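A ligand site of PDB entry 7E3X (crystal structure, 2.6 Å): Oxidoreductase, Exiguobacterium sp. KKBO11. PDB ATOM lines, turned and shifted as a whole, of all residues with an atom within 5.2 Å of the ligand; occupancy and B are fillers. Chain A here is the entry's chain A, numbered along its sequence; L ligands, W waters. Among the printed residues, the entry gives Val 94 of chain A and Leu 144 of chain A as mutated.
N of Glu 194 is in hydrogen-bond range of O1 of the ligand. N of Arg 39 sits at hydrogen-bond distance from O15 of the ligand, 2.7 Å away. A nitrogen (N4) of the ligand lies within hydrogen-bond range of the backbone NH (N) of Leu 67 (2.9 Å). OG of Ser 16 lies within hydrogen-bond range of O6 of the ligand. An oxygen (O2) of the ligand lies within salt-bridge range of the guanidinium group (NE) of Arg 198 (3.1 Å). O17 of the ligand sits at hydrogen-bond distance from N of Arg 40 (3.0 Å). O12 of the ligand lies within hydrogen-bond range of NZ of Lys 160 (2.9 Å). OG1 of Thr 193 is in hydrogen-bond range of O8 of the ligand, 2.8 Å away. NE of Arg 40 lies within salt-bridge range of O17 of the ligand. N7 of the ligand is in hydrogen-bond range of O of Thr 191 (2.9 Å). The backbone NH (N) of Ser 17 is in hydrogen-bond range of an oxygen (O5) of the ligand (3.4 Å). The guanidinium group (NH2) of Arg 39 is in salt-bridge range of an oxygen (O16) of the ligand, 2.8 Å away. The backbone NH of Ser 16 sits at hydrogen-bond distance from an oxygen (O5) of the ligand. The backbone carbonyl oxygen (O) of Asn 91 is in hydrogen-bond range of an oxygen (O12) of the ligand (3.0 Å). O5 of the ligand sits at hydrogen-bond distance from O of Gly 14, at 2.9 Å. N3 of the ligand is in hydrogen-bond range of OD1 of Asp 66 (3.2 Å). The side-chain hydroxyl of Tyr 156 is in hydrogen-bond range of an oxygen (O13) of the ligand (2.6 Å). OG of Ser 17 is in hydrogen-bond range of O1 of the ligand, 2.6 Å away. O1 of the ligand sits at hydrogen-bond distance from N of Gly 18 (3.4 Å). The backbone NH of Ile 19 is in hydrogen-bond range of an oxygen (O9) of the ligand (2.9 Å). The backbone NH (N) of Thr 191 sits at hydrogen-bond distance from an oxygen (O14) of the ligand, at 3.0 Å.
O of Gly 14 sits at hydrogen-bond distance from ND2 of Asn 91 (3.0 Å). NH1 of Arg 40 lies within salt-bridge range of OE1 of Glu 194 (2.9 Å). The backbone NH (N) of Gly 14 is in hydrogen-bond range of the backbone carbonyl oxygen (O) of Val 37 (2.6 Å). The backbone NH of Val 65 lies within hydrogen-bond range of the backbone carbonyl oxygen of Ala 38. The backbone carbonyl oxygen of Thr 191 sits at hydrogen-bond distance from the side-chain hydroxyl of Tyr 207, 3.2 Å away. The guanidinium group (NH2) of Arg 40 lies within hydrogen-bond range of the side-chain hydroxyl (OG) of Ser 16, at 3.1 Å. OG of Ser 17 sits at hydrogen-bond distance from NH2 of Arg 198 (3.1 Å). OE1 of Glu 194 is in salt-bridge range of NH2 of Arg 198.
An oxygen (O14) of the ligand sits close to the backbone carbonyl oxygen of Ala 189 (3.3 Å). Merely in contact with the ligand: Ala 15 (3.6 Å), Ala 38 (3.7 Å), Val 65 (3.4 Å), Ala 68 (3.8 Å), Ala 92 (3.6 Å), Gly 93 (3.7 Å), Val 94 (3.7 Å), Leu 114 (3.3 Å), Ile 141 (3.8 Å), Ser 142 (3.2 Å), Ser 143 (3.0 Å), Pro 188 (3.4 Å), Ala 190 (3.8 Å) and Phe 195 (3.4 Å). Of the 36 residues printed, 31 come within 4 Å of the ligand.
Water W1 lies within hydrogen-bond range of OG of Ser 143 (2.7 Å) and OH of Tyr 156 (2.9 Å).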
ATOM      1  N   GLY A  14     -10.967   9.373  18.210  1.00  0.00           N
ATOM      2  CA  GLY A  14     -10.467  10.418  19.077  1.00  0.00           C
ATOM      3  C   GLY A  14      -9.971  11.583  18.252  1.00  0.00           C
ATOM      4  O   GLY A  14      -8.895  12.126  18.525  1.00  0.00           O
ATOM      5  N   ALA A  15     -10.755  11.958  17.255  1.00  0.00           N
ATOM      6  CA  ALA A  15     -10.387  12.975  16.280  1.00  0.00           C
ATOM      7  C   ALA A  15     -10.794  14.384  16.700  1.00  0.00           C
ATOM      8  O   ALA A  15     -10.407  15.348  16.020  1.00  0.00           O
ATOM      9  CB  ALA A  15     -11.035  12.650  14.933  1.00  0.00           C
ATOM     10  N   SER A  16     -11.548  14.513  17.777  1.00  0.00           N
ATOM     11  CA  SER A  16     -12.159  15.775  18.150  1.00  0.00           C
ATOM     12  C   SER A  16     -11.197  16.700  18.871  1.00  0.00           C
ATOM     13  O   SER A  16     -11.549  17.864  19.123  1.00  0.00           O
ATOM     14  CB  SER A  16     -13.373  15.532  19.035  1.00  0.00           C
ATOM     15  OG  SER A  16     -13.079  14.614  20.086  1.00  0.00           O
ATOM     16  N   SER A  17     -10.005  16.202  19.201  1.00  0.00           N
ATOM     17  CA  SER A  17      -8.987  16.976  19.892  1.00  0.00           C
ATOM     18  C   SER A  17      -7.649  16.265  19.749  1.00  0.00           C
ATOM     19  O   SER A  17      -7.566  15.135  19.261  1.00  0.00           O
ATOM     20  CB  SER A  17      -9.371  17.204  21.355  1.00  0.00           C
ATOM     21  OG  SER A  17      -8.956  16.119  22.151  1.00  0.00           O
ATOM     22  N   GLY A  18      -6.602  16.956  20.197  1.00  0.00           N
ATOM     23  CA  GLY A  18      -5.245  16.489  20.328  1.00  0.00           C
ATOM     24  C   GLY A  18      -4.703  15.832  19.065  1.00  0.00           C
ATOM     25  O   GLY A  18      -5.019  16.220  17.929  1.00  0.00           O
ATOM     26  N   ILE A  19      -3.890  14.800  19.295  1.00  0.00           N
ATOM     27  CA  ILE A  19      -3.153  14.128  18.226  1.00  0.00           C
ATOM     28  C   ILE A  19      -4.082  13.751  17.082  1.00  0.00           C
ATOM     29  O   ILE A  19      -3.770  13.984  15.899  1.00  0.00           O
ATOM     30  CB  ILE A  19      -2.424  12.900  18.787  1.00  0.00           C
ATOM     31  CG1 ILE A  19      -1.323  13.339  19.760  1.00  0.00           C
ATOM     32  CG2 ILE A  19      -1.855  12.048  17.637  1.00  0.00           C
ATOM     33  CD1 ILE A  19      -0.781  12.251  20.658  1.00  0.00           C
ATOM     34  N   GLY A  20      -5.224  13.154  17.403  1.00  0.00           N
ATOM     35  CA  GLY A  20      -6.101  12.680  16.348  1.00  0.00           C
ATOM     36  C   GLY A  20      -6.665  13.801  15.500  1.00  0.00           C
ATOM     37  O   GLY A  20      -6.940  13.609  14.312  1.00  0.00           O
ATOM     38  N   VAL A  37     -13.981   9.837  14.418  1.00  0.00           N
ATOM     39  CA  VAL A  37     -14.783   9.224  15.473  1.00  0.00           C
ATOM     40  C   VAL A  37     -14.403   9.846  16.803  1.00  0.00           C
ATOM     41  O   VAL A  37     -13.219   9.989  17.117  1.00  0.00           O
ATOM     42  CB  VAL A  37     -14.591   7.700  15.511  1.00  0.00           C
ATOM     43  CG1 VAL A  37     -15.591   7.076  16.462  1.00  0.00           C
ATOM     44  CG2 VAL A  37     -14.763   7.120  14.112  1.00  0.00           C
ATOM     45  N   ALA A  38     -15.422  10.205  17.593  1.00  0.00           N
ATOM     46  CA  ALA A  38     -15.270  10.805  18.914  1.00  0.00           C
ATOM     47  C   ALA A  38     -16.649  11.024  19.538  1.00  0.00           C
ATOM     48  O   ALA A  38     -17.670  10.746  18.891  1.00  0.00           O
ATOM     49  CB  ALA A  38     -14.512  12.132  18.840  1.00  0.00           C
ATOM     50  N   ARG A  39     -16.696  11.531  20.767  1.00  0.00           N
ATOM     51  CA  ARG A  39     -18.011  11.754  21.357  1.00  0.00           C
ATOM     52  C   ARG A  39     -18.535  13.159  21.057  1.00  0.00           C
ATOM     53  O   ARG A  39     -19.723  13.320  20.765  1.00  0.00           O
ATOM     54  CB  ARG A  39     -17.954  11.502  22.860  1.00  0.00           C
ATOM     55  CG  ARG A  39     -17.818  10.040  23.236  1.00  0.00           C
ATOM     56  CD  ARG A  39     -17.449   9.899  24.700  1.00  0.00           C
ATOM     57  NE  ARG A  39     -16.301  10.750  24.986  1.00  0.00           N
ATOM     58  CZ  ARG A  39     -15.843  10.995  26.204  1.00  0.00           C
ATOM     59  NH1 ARG A  39     -16.423  10.435  27.237  1.00  0.00           N
ATOM     60  NH2 ARG A  39     -14.791  11.783  26.359  1.00  0.00           N
ATOM     61  N   ARG A  40     -17.680  14.182  21.105  1.00  0.00           N
ATOM     62  CA  ARG A  40     -18.097  15.560  20.918  1.00  0.00           C
ATOM     63  C   ARG A  40     -18.425  15.893  19.456  1.00  0.00           C
ATOM     64  O   ARG A  40     -17.536  16.281  18.709  1.00  0.00           O
ATOM     65  CB  ARG A  40     -17.013  16.521  21.407  1.00  0.00           C
ATOM     66  CG  ARG A  40     -16.886  16.526  22.919  1.00  0.00           C
ATOM     67  CD  ARG A  40     -15.619  17.197  23.358  1.00  0.00           C
ATOM     68  NE  ARG A  40     -14.455  16.461  22.876  1.00  0.00           N
ATOM     69  CZ  ARG A  40     -13.204  16.813  23.138  1.00  0.00           C
ATOM     70  NH1 ARG A  40     -12.954  17.880  23.879  1.00  0.00           N
ATOM     71  NH2 ARG A  40     -12.195  16.099  22.664  1.00  0.00           N
ATOM     72  N   VAL A  65     -19.539   8.604  18.715  1.00  0.00           N
ATOM     73  CA  VAL A  65     -19.633   7.309  19.385  1.00  0.00           C
ATOM     74  C   VAL A  65     -18.880   7.379  20.706  1.00  0.00           C
ATOM     75  O   VAL A  65     -17.774   7.938  20.779  1.00  0.00           O
ATOM     76  CB  VAL A  65     -19.066   6.166  18.529  1.00  0.00           C
ATOM     77  CG1 VAL A  65     -19.463   4.829  19.102  1.00  0.00           C
ATOM     78  CG2 VAL A  65     -19.538   6.287  17.094  1.00  0.00           C
ATOM     79  N   ASP A  66     -19.455   6.789  21.738  1.00  0.00           N
ATOM     80  CA  ASP A  66     -18.707   6.518  22.956  1.00  0.00           C
ATOM     81  C   ASP A  66     -18.157   5.100  22.821  1.00  0.00           C
ATOM     82  O   ASP A  66     -18.922   4.132  22.828  1.00  0.00           O
ATOM     83  CB  ASP A  66     -19.583   6.687  24.189  1.00  0.00           C
ATOM     84  CG  ASP A  66     -18.876   6.282  25.475  1.00  0.00           C
ATOM     85  OD1 ASP A  66     -17.822   5.615  25.429  1.00  0.00           O
ATOM     86  OD2 ASP A  66     -19.382   6.650  26.549  1.00  0.00           O
ATOM     87  N   LEU A  67     -16.830   4.997  22.689  1.00  0.00           N
ATOM     88  CA  LEU A  67     -16.142   3.744  22.435  1.00  0.00           C
ATOM     89  C   LEU A  67     -15.763   3.003  23.721  1.00  0.00           C
ATOM     90  O   LEU A  67     -15.105   1.958  23.649  1.00  0.00           O
ATOM     91  CB  LEU A  67     -14.891   4.001  21.594  1.00  0.00           C
ATOM     92  CG  LEU A  67     -15.075   4.472  20.139  1.00  0.00           C
ATOM     93  CD1 LEU A  67     -13.741   4.955  19.548  1.00  0.00           C
ATOM     94  CD2 LEU A  67     -15.659   3.358  19.302  1.00  0.00           C
ATOM     95  N   ALA A  68     -16.159   3.499  24.884  1.00  0.00           N
ATOM     96  CA  ALA A  68     -16.033   2.734  26.111  1.00  0.00           C
ATOM     97  C   ALA A  68     -17.135   1.686  26.248  1.00  0.00           C
ATOM     98  O   ALA A  68     -17.187   0.981  27.269  1.00  0.00           O
ATOM     99  CB  ALA A  68     -16.028   3.680  27.310  1.00  0.00           C
ATOM    100  N   ASN A  91      -6.632   5.894  17.984  1.00  0.00           N
ATOM    101  CA  ASN A  91      -6.019   6.997  18.734  1.00  0.00           C
ATOM    102  C   ASN A  91      -6.788   7.378  19.992  1.00  0.00           C
ATOM    103  O   ASN A  91      -6.169   7.913  20.923  1.00  0.00           O
ATOM    104  CB  ASN A  91      -5.852   8.229  17.806  1.00  0.00           C
ATOM    105  CG  ASN A  91      -5.468   9.514  18.548  1.00  0.00           C
ATOM    106  OD1 ASN A  91      -4.344   9.658  19.012  1.00  0.00           O
ATOM    107  ND2 ASN A  91      -6.383  10.471  18.605  1.00  0.00           N
ATOM    108  N   ALA A  92      -8.087   7.101  20.070  1.00  0.00           N
ATOM    109  CA  ALA A  92      -8.868   7.567  21.218  1.00  0.00           C
ATOM    110  C   ALA A  92      -8.422   6.850  22.484  1.00  0.00           C
ATOM    111  O   ALA A  92      -8.234   5.622  22.480  1.00  0.00           O
ATOM    112  CB  ALA A  92     -10.360   7.343  20.979  1.00  0.00           C
ATOM    113  N   GLY A  93      -8.239   7.611  23.559  1.00  0.00           N
ATOM    114  CA  GLY A  93      -7.736   7.089  24.812  1.00  0.00           C
ATOM    115  C   GLY A  93      -7.728   8.165  25.868  1.00  0.00           C
ATOM    116  O   GLY A  93      -7.715   9.365  25.562  1.00  0.00           O
ATOM    117  N   VAL A  94      -7.740   7.730  27.120  1.00  0.00           N
ATOM    118  CA  VAL A  94      -7.739   8.638  28.251  1.00  0.00           C
ATOM    119  C   VAL A  94      -6.744   8.137  29.288  1.00  0.00           C
ATOM    120  O   VAL A  94      -6.364   6.965  29.285  1.00  0.00           O
ATOM    121  CB  VAL A  94      -9.137   8.792  28.871  1.00  0.00           C
ATOM    122  CG1 VAL A  94     -10.093   9.440  27.904  1.00  0.00           C
ATOM    123  CG2 VAL A  94      -9.650   7.453  29.282  1.00  0.00           C
ATOM    124  N   LEU A 114     -12.055   1.648  26.954  1.00  0.00           N
ATOM    125  CA  LEU A 114     -11.591   2.465  25.850  1.00  0.00           C
ATOM    126  C   LEU A 114     -10.183   2.078  25.417  1.00  0.00           C
ATOM    127  O   LEU A 114      -9.969   1.700  24.264  1.00  0.00           O
ATOM    128  CB  LEU A 114     -11.646   3.953  26.228  1.00  0.00           C
ATOM    129  CG  LEU A 114     -11.130   4.921  25.146  1.00  0.00           C
ATOM    130  CD1 LEU A 114     -12.027   4.902  23.882  1.00  0.00           C
ATOM    131  CD2 LEU A 114     -10.991   6.365  25.673  1.00  0.00           C
ATOM    132  N   ILE A 141      -2.136   3.765  18.986  1.00  0.00           N
ATOM    133  CA  ILE A 141      -1.440   4.825  19.704  1.00  0.00           C
ATOM    134  C   ILE A 141      -1.200   4.376  21.137  1.00  0.00           C
ATOM    135  O   ILE A 141      -2.130   4.292  21.947  1.00  0.00           O
ATOM    136  CB  ILE A 141      -2.206   6.142  19.636  1.00  0.00           C
ATOM    137  CG1 ILE A 141      -2.515   6.478  18.180  1.00  0.00           C
ATOM    138  CG2 ILE A 141      -1.425   7.260  20.323  1.00  0.00           C
ATOM    139  CD1 ILE A 141      -1.292   6.589  17.304  1.00  0.00           C
ATOM    140  N   SER A 142       0.057   4.074  21.456  1.00  0.00           N
ATOM    141  CA  SER A 142       0.422   3.673  22.806  1.00  0.00           C
ATOM    142  C   SER A 142       0.931   4.922  23.508  1.00  0.00           C
ATOM    143  O   SER A 142       0.270   5.961  23.494  1.00  0.00           O
ATOM    144  CB  SER A 142       1.457   2.544  22.766  1.00  0.00           C
ATOM    145  OG  SER A 142       1.847   2.161  24.063  1.00  0.00           O
ATOM    146  N   SER A 143       2.114   4.847  24.103  1.00  0.00           N
ATOM    147  CA  SER A 143       2.758   5.971  24.749  1.00  0.00           C
ATOM    148  C   SER A 143       4.134   5.472  25.167  1.00  0.00           C
ATOM    149  O   SER A 143       4.329   4.268  25.325  1.00  0.00           O
ATOM    150  CB  SER A 143       1.972   6.453  25.971  1.00  0.00           C
ATOM    151  OG  SER A 143       2.654   7.479  26.681  1.00  0.00           O
ATOM    152  N   LEU A 144       5.074   6.411  25.357  1.00  0.00           N
ATOM    153  CA  LEU A 144       6.292   6.030  26.066  1.00  0.00           C
ATOM    154  C   LEU A 144       5.944   5.366  27.390  1.00  0.00           C
ATOM    155  O   LEU A 144       6.706   4.524  27.877  1.00  0.00           O
ATOM    156  CB  LEU A 144       7.221   7.241  26.282  1.00  0.00           C
ATOM    157  CG  LEU A 144       8.621   6.970  26.901  1.00  0.00           C
ATOM    158  CD1 LEU A 144       9.460   6.020  26.054  1.00  0.00           C
ATOM    159  CD2 LEU A 144       9.389   8.262  27.140  1.00  0.00           C
ATOM    160  N   TYR A 156      -2.957   3.396  33.844  1.00  0.00           N
ATOM    161  CA  TYR A 156      -2.904   3.886  32.474  1.00  0.00           C
ATOM    162  C   TYR A 156      -1.704   3.282  31.744  1.00  0.00           C
ATOM    163  O   TYR A 156      -1.849   2.712  30.649  1.00  0.00           O
ATOM    164  CB  TYR A 156      -2.845   5.406  32.449  1.00  0.00           C
ATOM    165  CG  TYR A 156      -2.418   5.994  31.119  1.00  0.00           C
ATOM    166  CD1 TYR A 156      -3.303   6.078  30.060  1.00  0.00           C
ATOM    167  CD2 TYR A 156      -1.132   6.487  30.935  1.00  0.00           C
ATOM    168  CE1 TYR A 156      -2.927   6.620  28.846  1.00  0.00           C
ATOM    169  CE2 TYR A 156      -0.744   7.032  29.715  1.00  0.00           C
ATOM    170  CZ  TYR A 156      -1.642   7.103  28.671  1.00  0.00           C
ATOM    171  OH  TYR A 156      -1.257   7.646  27.461  1.00  0.00           O
ATOM    172  N   LYS A 160      -1.227   1.037  28.321  1.00  0.00           N
ATOM    173  CA  LYS A 160      -0.366   1.298  27.172  1.00  0.00           C
ATOM    174  C   LYS A 160       0.651   0.195  26.972  1.00  0.00           C
ATOM    175  O   LYS A 160       1.064  -0.055  25.830  1.00  0.00           O
ATOM    176  CB  LYS A 160       0.333   2.643  27.333  1.00  0.00           C
ATOM    177  CG  LYS A 160      -0.588   3.830  27.256  1.00  0.00           C
ATOM    178  CD  LYS A 160      -1.492   3.714  26.063  1.00  0.00           C
ATOM    179  CE  LYS A 160      -2.375   4.953  25.909  1.00  0.00           C
ATOM    180  NZ  LYS A 160      -2.882   5.096  24.508  1.00  0.00           N
ATOM    181  N   PRO A 188       4.102   8.344  21.793  1.00  0.00           N
ATOM    182  CA  PRO A 188       4.417   9.754  22.054  1.00  0.00           C
ATOM    183  C   PRO A 188       4.912  10.025  23.476  1.00  0.00           C
ATOM    184  O   PRO A 188       4.735   9.183  24.328  1.00  0.00           O
ATOM    185  CB  PRO A 188       3.069  10.468  21.900  1.00  0.00           C
ATOM    186  CG  PRO A 188       2.189   9.497  21.178  1.00  0.00           C
ATOM    187  CD  PRO A 188       2.674   8.139  21.608  1.00  0.00           C
ATOM    188  N   ALA A 189       5.475  11.208  23.715  1.00  0.00           N
ATOM    189  CA  ALA A 189       5.960  11.542  25.066  1.00  0.00           C
ATOM    190  C   ALA A 189       5.031  12.658  25.547  1.00  0.00           C
ATOM    191  O   ALA A 189       3.833  12.560  25.286  1.00  0.00           O
ATOM    192  CB  ALA A 189       7.401  11.976  25.028  1.00  0.00           C
ATOM    193  N   ALA A 190       5.530  13.682  26.232  1.00  0.00           N
ATOM    194  CA  ALA A 190       4.567  14.726  26.589  1.00  0.00           C
ATOM    195  C   ALA A 190       4.117  15.374  25.272  1.00  0.00           C
ATOM    196  O   ALA A 190       4.978  15.830  24.512  1.00  0.00           O
ATOM    197  CB  ALA A 190       5.194  15.721  27.520  1.00  0.00           C
ATOM    198  N   THR A 191       2.813  15.379  25.021  1.00  0.00           N
ATOM    199  CA  THR A 191       2.247  15.951  23.776  1.00  0.00           C
ATOM    200  C   THR A 191       1.163  16.959  24.197  1.00  0.00           C
ATOM    201  O   THR A 191       0.271  16.580  24.945  1.00  0.00           O
ATOM    202  CB  THR A 191       1.739  14.868  22.819  1.00  0.00           C
ATOM    203  OG1 THR A 191       2.856  14.100  22.402  1.00  0.00           O
ATOM    204  CG2 THR A 191       1.083  15.442  21.588  1.00  0.00           C
ATOM    205  N   GLU A 192       1.265  18.186  23.701  1.00  0.00           N
ATOM    206  CA  GLU A 192       0.338  19.246  24.070  1.00  0.00           C
ATOM    207  C   GLU A 192      -1.043  18.938  23.499  1.00  0.00           C
ATOM    208  O   GLU A 192      -1.308  19.175  22.319  1.00  0.00           O
ATOM    209  CB  GLU A 192       0.856  20.591  23.577  1.00  0.00           C
ATOM    210  CG  GLU A 192       0.049  21.752  24.015  1.00  0.00           C
ATOM    211  CD  GLU A 192       0.653  23.051  23.543  1.00  0.00           C
ATOM    212  OE1 GLU A 192       0.900  23.161  22.327  1.00  0.00           O
ATOM    213  OE2 GLU A 192       0.895  23.947  24.399  1.00  0.00           O
ATOM    214  N   THR A 193      -1.901  18.366  24.342  1.00  0.00           N
ATOM    215  CA  THR A 193      -3.259  18.001  23.960  1.00  0.00           C
ATOM    216  C   THR A 193      -4.163  18.268  25.165  1.00  0.00           C
ATOM    217  O   THR A 193      -3.767  18.933  26.126  1.00  0.00           O
ATOM    218  CB  THR A 193      -3.369  16.527  23.523  1.00  0.00           C
ATOM    219  OG1 THR A 193      -3.184  15.666  24.652  1.00  0.00           O
ATOM    220  CG2 THR A 193      -2.339  16.195  22.455  1.00  0.00           C
ATOM    221  N   GLU A 194      -5.375  17.729  25.114  1.00  0.00           N
ATOM    222  CA  GLU A 194      -6.292  17.784  26.238  1.00  0.00           C
ATOM    223  C   GLU A 194      -6.082  16.641  27.207  1.00  0.00           C
ATOM    224  O   GLU A 194      -6.816  16.553  28.203  1.00  0.00           O
ATOM    225  CB  GLU A 194      -7.737  17.807  25.726  1.00  0.00           C
ATOM    226  CG  GLU A 194      -8.053  19.063  24.926  1.00  0.00           C
ATOM    227  CD  GLU A 194      -9.496  19.144  24.474  1.00  0.00           C
ATOM    228  OE1 GLU A 194     -10.210  18.138  24.608  1.00  0.00           O
ATOM    229  OE2 GLU A 194      -9.921  20.212  23.978  1.00  0.00           O
ATOM    230  N   PHE A 195      -5.090  15.790  26.954  1.00  0.00           N
ATOM    231  CA  PHE A 195      -4.922  14.549  27.710  1.00  0.00           C
ATOM    232  C   PHE A 195      -4.843  14.810  29.203  1.00  0.00           C
ATOM    233  O   PHE A 195      -5.540  14.150  29.990  1.00  0.00           O
ATOM    234  CB  PHE A 195      -3.670  13.810  27.222  1.00  0.00           C
ATOM    235  CG  PHE A 195      -3.379  12.560  27.994  1.00  0.00           C
ATOM    236  CD1 PHE A 195      -3.952  11.352  27.634  1.00  0.00           C
ATOM    237  CD2 PHE A 195      -2.520  12.581  29.078  1.00  0.00           C
ATOM    238  CE1 PHE A 195      -3.677  10.184  28.346  1.00  0.00           C
ATOM    239  CE2 PHE A 195      -2.232  11.416  29.785  1.00  0.00           C
ATOM    240  CZ  PHE A 195      -2.823  10.215  29.409  1.00  0.00           C
ATOM    241  N   ARG A 198      -8.192  15.890  30.696  1.00  0.00           N
ATOM    242  CA  ARG A 198      -9.170  14.795  30.803  1.00  0.00           C
ATOM    243  C   ARG A 198      -8.814  13.825  31.919  1.00  0.00           C
ATOM    244  O   ARG A 198      -9.695  13.319  32.604  1.00  0.00           O
ATOM    245  CB  ARG A 198      -9.296  14.037  29.483  1.00  0.00           C
ATOM    246  CG  ARG A 198     -10.581  14.342  28.819  1.00  0.00           C
ATOM    247  CD  ARG A 198     -10.934  13.388  27.713  1.00  0.00           C
ATOM    248  NE  ARG A 198     -10.538  13.958  26.424  1.00  0.00           N
ATOM    249  CZ  ARG A 198     -10.960  15.128  25.930  1.00  0.00           C
ATOM    250  NH1 ARG A 198     -11.829  15.899  26.569  1.00  0.00           N
ATOM    251  NH2 ARG A 198     -10.490  15.532  24.762  1.00  0.00           N
ATOM    252  N   TYR A 207       0.906  23.492  29.367  1.00  0.00           N
ATOM    253  CA  TYR A 207       2.162  22.827  29.026  1.00  0.00           C
ATOM    254  C   TYR A 207       3.317  23.821  28.952  1.00  0.00           C
ATOM    255  O   TYR A 207       4.420  23.531  29.446  1.00  0.00           O
ATOM    256  CB  TYR A 207       2.016  22.076  27.700  1.00  0.00           C
ATOM    257  CG  TYR A 207       1.273  20.753  27.759  1.00  0.00           C
ATOM    258  CD1 TYR A 207      -0.121  20.701  27.685  1.00  0.00           C
ATOM    259  CD2 TYR A 207       1.958  19.539  27.888  1.00  0.00           C
ATOM    260  CE1 TYR A 207      -0.805  19.510  27.756  1.00  0.00           C
ATOM    261  CE2 TYR A 207       1.275  18.330  27.935  1.00  0.00           C
ATOM    262  CZ  TYR A 207      -0.103  18.330  27.883  1.00  0.00           C
ATOM    263  OH  TYR A 207      -0.760  17.135  27.940  1.00  0.00           O
HETATM  264  P1  LIG L   1      -6.962  14.367  23.976  1.00  0.00           P
HETATM  265  O1  LIG L   1      -6.706  15.718  23.404  1.00  0.00           O
HETATM  266  O2  LIG L   1      -7.734  14.247  25.241  1.00  0.00           O
HETATM  267  O3  LIG L   1      -7.650  13.452  22.866  1.00  0.00           O
HETATM  268  C1  LIG L   1      -8.239  12.164  23.187  1.00  0.00           C
HETATM  269  C2  LIG L   1      -9.318  11.864  22.172  1.00  0.00           C
HETATM  270  O4  LIG L   1     -10.038  10.679  22.580  1.00  0.00           O
HETATM  271  C3  LIG L   1     -10.375  12.959  22.002  1.00  0.00           C
HETATM  272  O5  LIG L   1     -10.660  13.172  20.635  1.00  0.00           O
HETATM  273  C4  LIG L   1     -11.604  12.387  22.710  1.00  0.00           C
HETATM  274  O6  LIG L   1     -12.739  12.963  22.069  1.00  0.00           O
HETATM  275  C5  LIG L   1     -11.421  10.909  22.424  1.00  0.00           C
HETATM  276  N1  LIG L   1     -12.143  10.052  23.361  1.00  0.00           N
HETATM  277  C6  LIG L   1     -11.966  10.003  24.713  1.00  0.00           C
HETATM  278  N2  LIG L   1     -12.752   9.153  25.315  1.00  0.00           N
HETATM  279  C7  LIG L   1     -13.498   8.599  24.291  1.00  0.00           C
HETATM  280  C8  LIG L   1     -14.522   7.625  24.281  1.00  0.00           C
HETATM  281  N3  LIG L   1     -14.975   7.024  25.370  1.00  0.00           N
HETATM  282  N4  LIG L   1     -15.069   7.301  23.080  1.00  0.00           N
HETATM  283  C9  LIG L   1     -14.614   7.913  21.982  1.00  0.00           C
HETATM  284  N5  LIG L   1     -13.663   8.839  21.881  1.00  0.00           N
HETATM  285  C10 LIG L   1     -13.143   9.148  23.072  1.00  0.00           C
HETATM  286  O7  LIG L   1      -5.548  13.651  24.193  1.00  0.00           O
HETATM  287  P2  LIG L   1      -4.442  12.991  23.228  1.00  0.00           P
HETATM  288  O8  LIG L   1      -3.157  12.999  23.957  1.00  0.00           O
HETATM  289  O9  LIG L   1      -4.527  13.647  21.897  1.00  0.00           O
HETATM  290  O10 LIG L   1      -4.996  11.488  23.125  1.00  0.00           O
HETATM  291  C11 LIG L   1      -4.706  10.687  21.958  1.00  0.00           C
HETATM  292  C12 LIG L   1      -3.839   9.515  22.326  1.00  0.00           C
HETATM  293  O11 LIG L   1      -2.523   9.986  22.684  1.00  0.00           O
HETATM  294  C13 LIG L   1      -4.294   8.654  23.522  1.00  0.00           C
HETATM  295  O12 LIG L   1      -4.217   7.293  23.143  1.00  0.00           O
HETATM  296  C14 LIG L   1      -3.200   8.966  24.552  1.00  0.00           C
HETATM  297  O13 LIG L   1      -3.052   7.983  25.562  1.00  0.00           O
HETATM  298  C15 LIG L   1      -1.984   9.098  23.655  1.00  0.00           C
HETATM  299  N6  LIG L   1      -0.820   9.748  24.324  1.00  0.00           N
HETATM  300  C16 LIG L   1      -0.877  11.072  24.694  1.00  0.00           C
HETATM  301  C17 LIG L   1       0.237  11.677  25.279  1.00  0.00           C
HETATM  302  C18 LIG L   1       0.154  13.114  25.737  1.00  0.00           C
HETATM  303  O14 LIG L   1       0.981  13.530  26.551  1.00  0.00           O
HETATM  304  N7  LIG L   1      -0.789  13.872  25.228  1.00  0.00           N
HETATM  305  C19 LIG L   1       1.405  10.961  25.399  1.00  0.00           C
HETATM  306  C20 LIG L   1       1.441   9.643  25.024  1.00  0.00           C
HETATM  307  C21 LIG L   1       0.309   9.041  24.528  1.00  0.00           C
HETATM  308  P3  LIG L   1     -14.158  13.015  22.840  1.00  0.00           P
HETATM  309  O15 LIG L   1     -14.858  11.677  22.742  1.00  0.00           O
HETATM  310  O16 LIG L   1     -13.844  13.374  24.279  1.00  0.00           O
HETATM  311  O17 LIG L   1     -14.910  14.115  22.121  1.00  0.00           O
HETATM  312  O   HOH W   1       1.102   9.105  28.225  1.00  0.00           O
HETATM  313  O   HOH W   2      -6.372  12.786  19.925  1.00  0.00           O
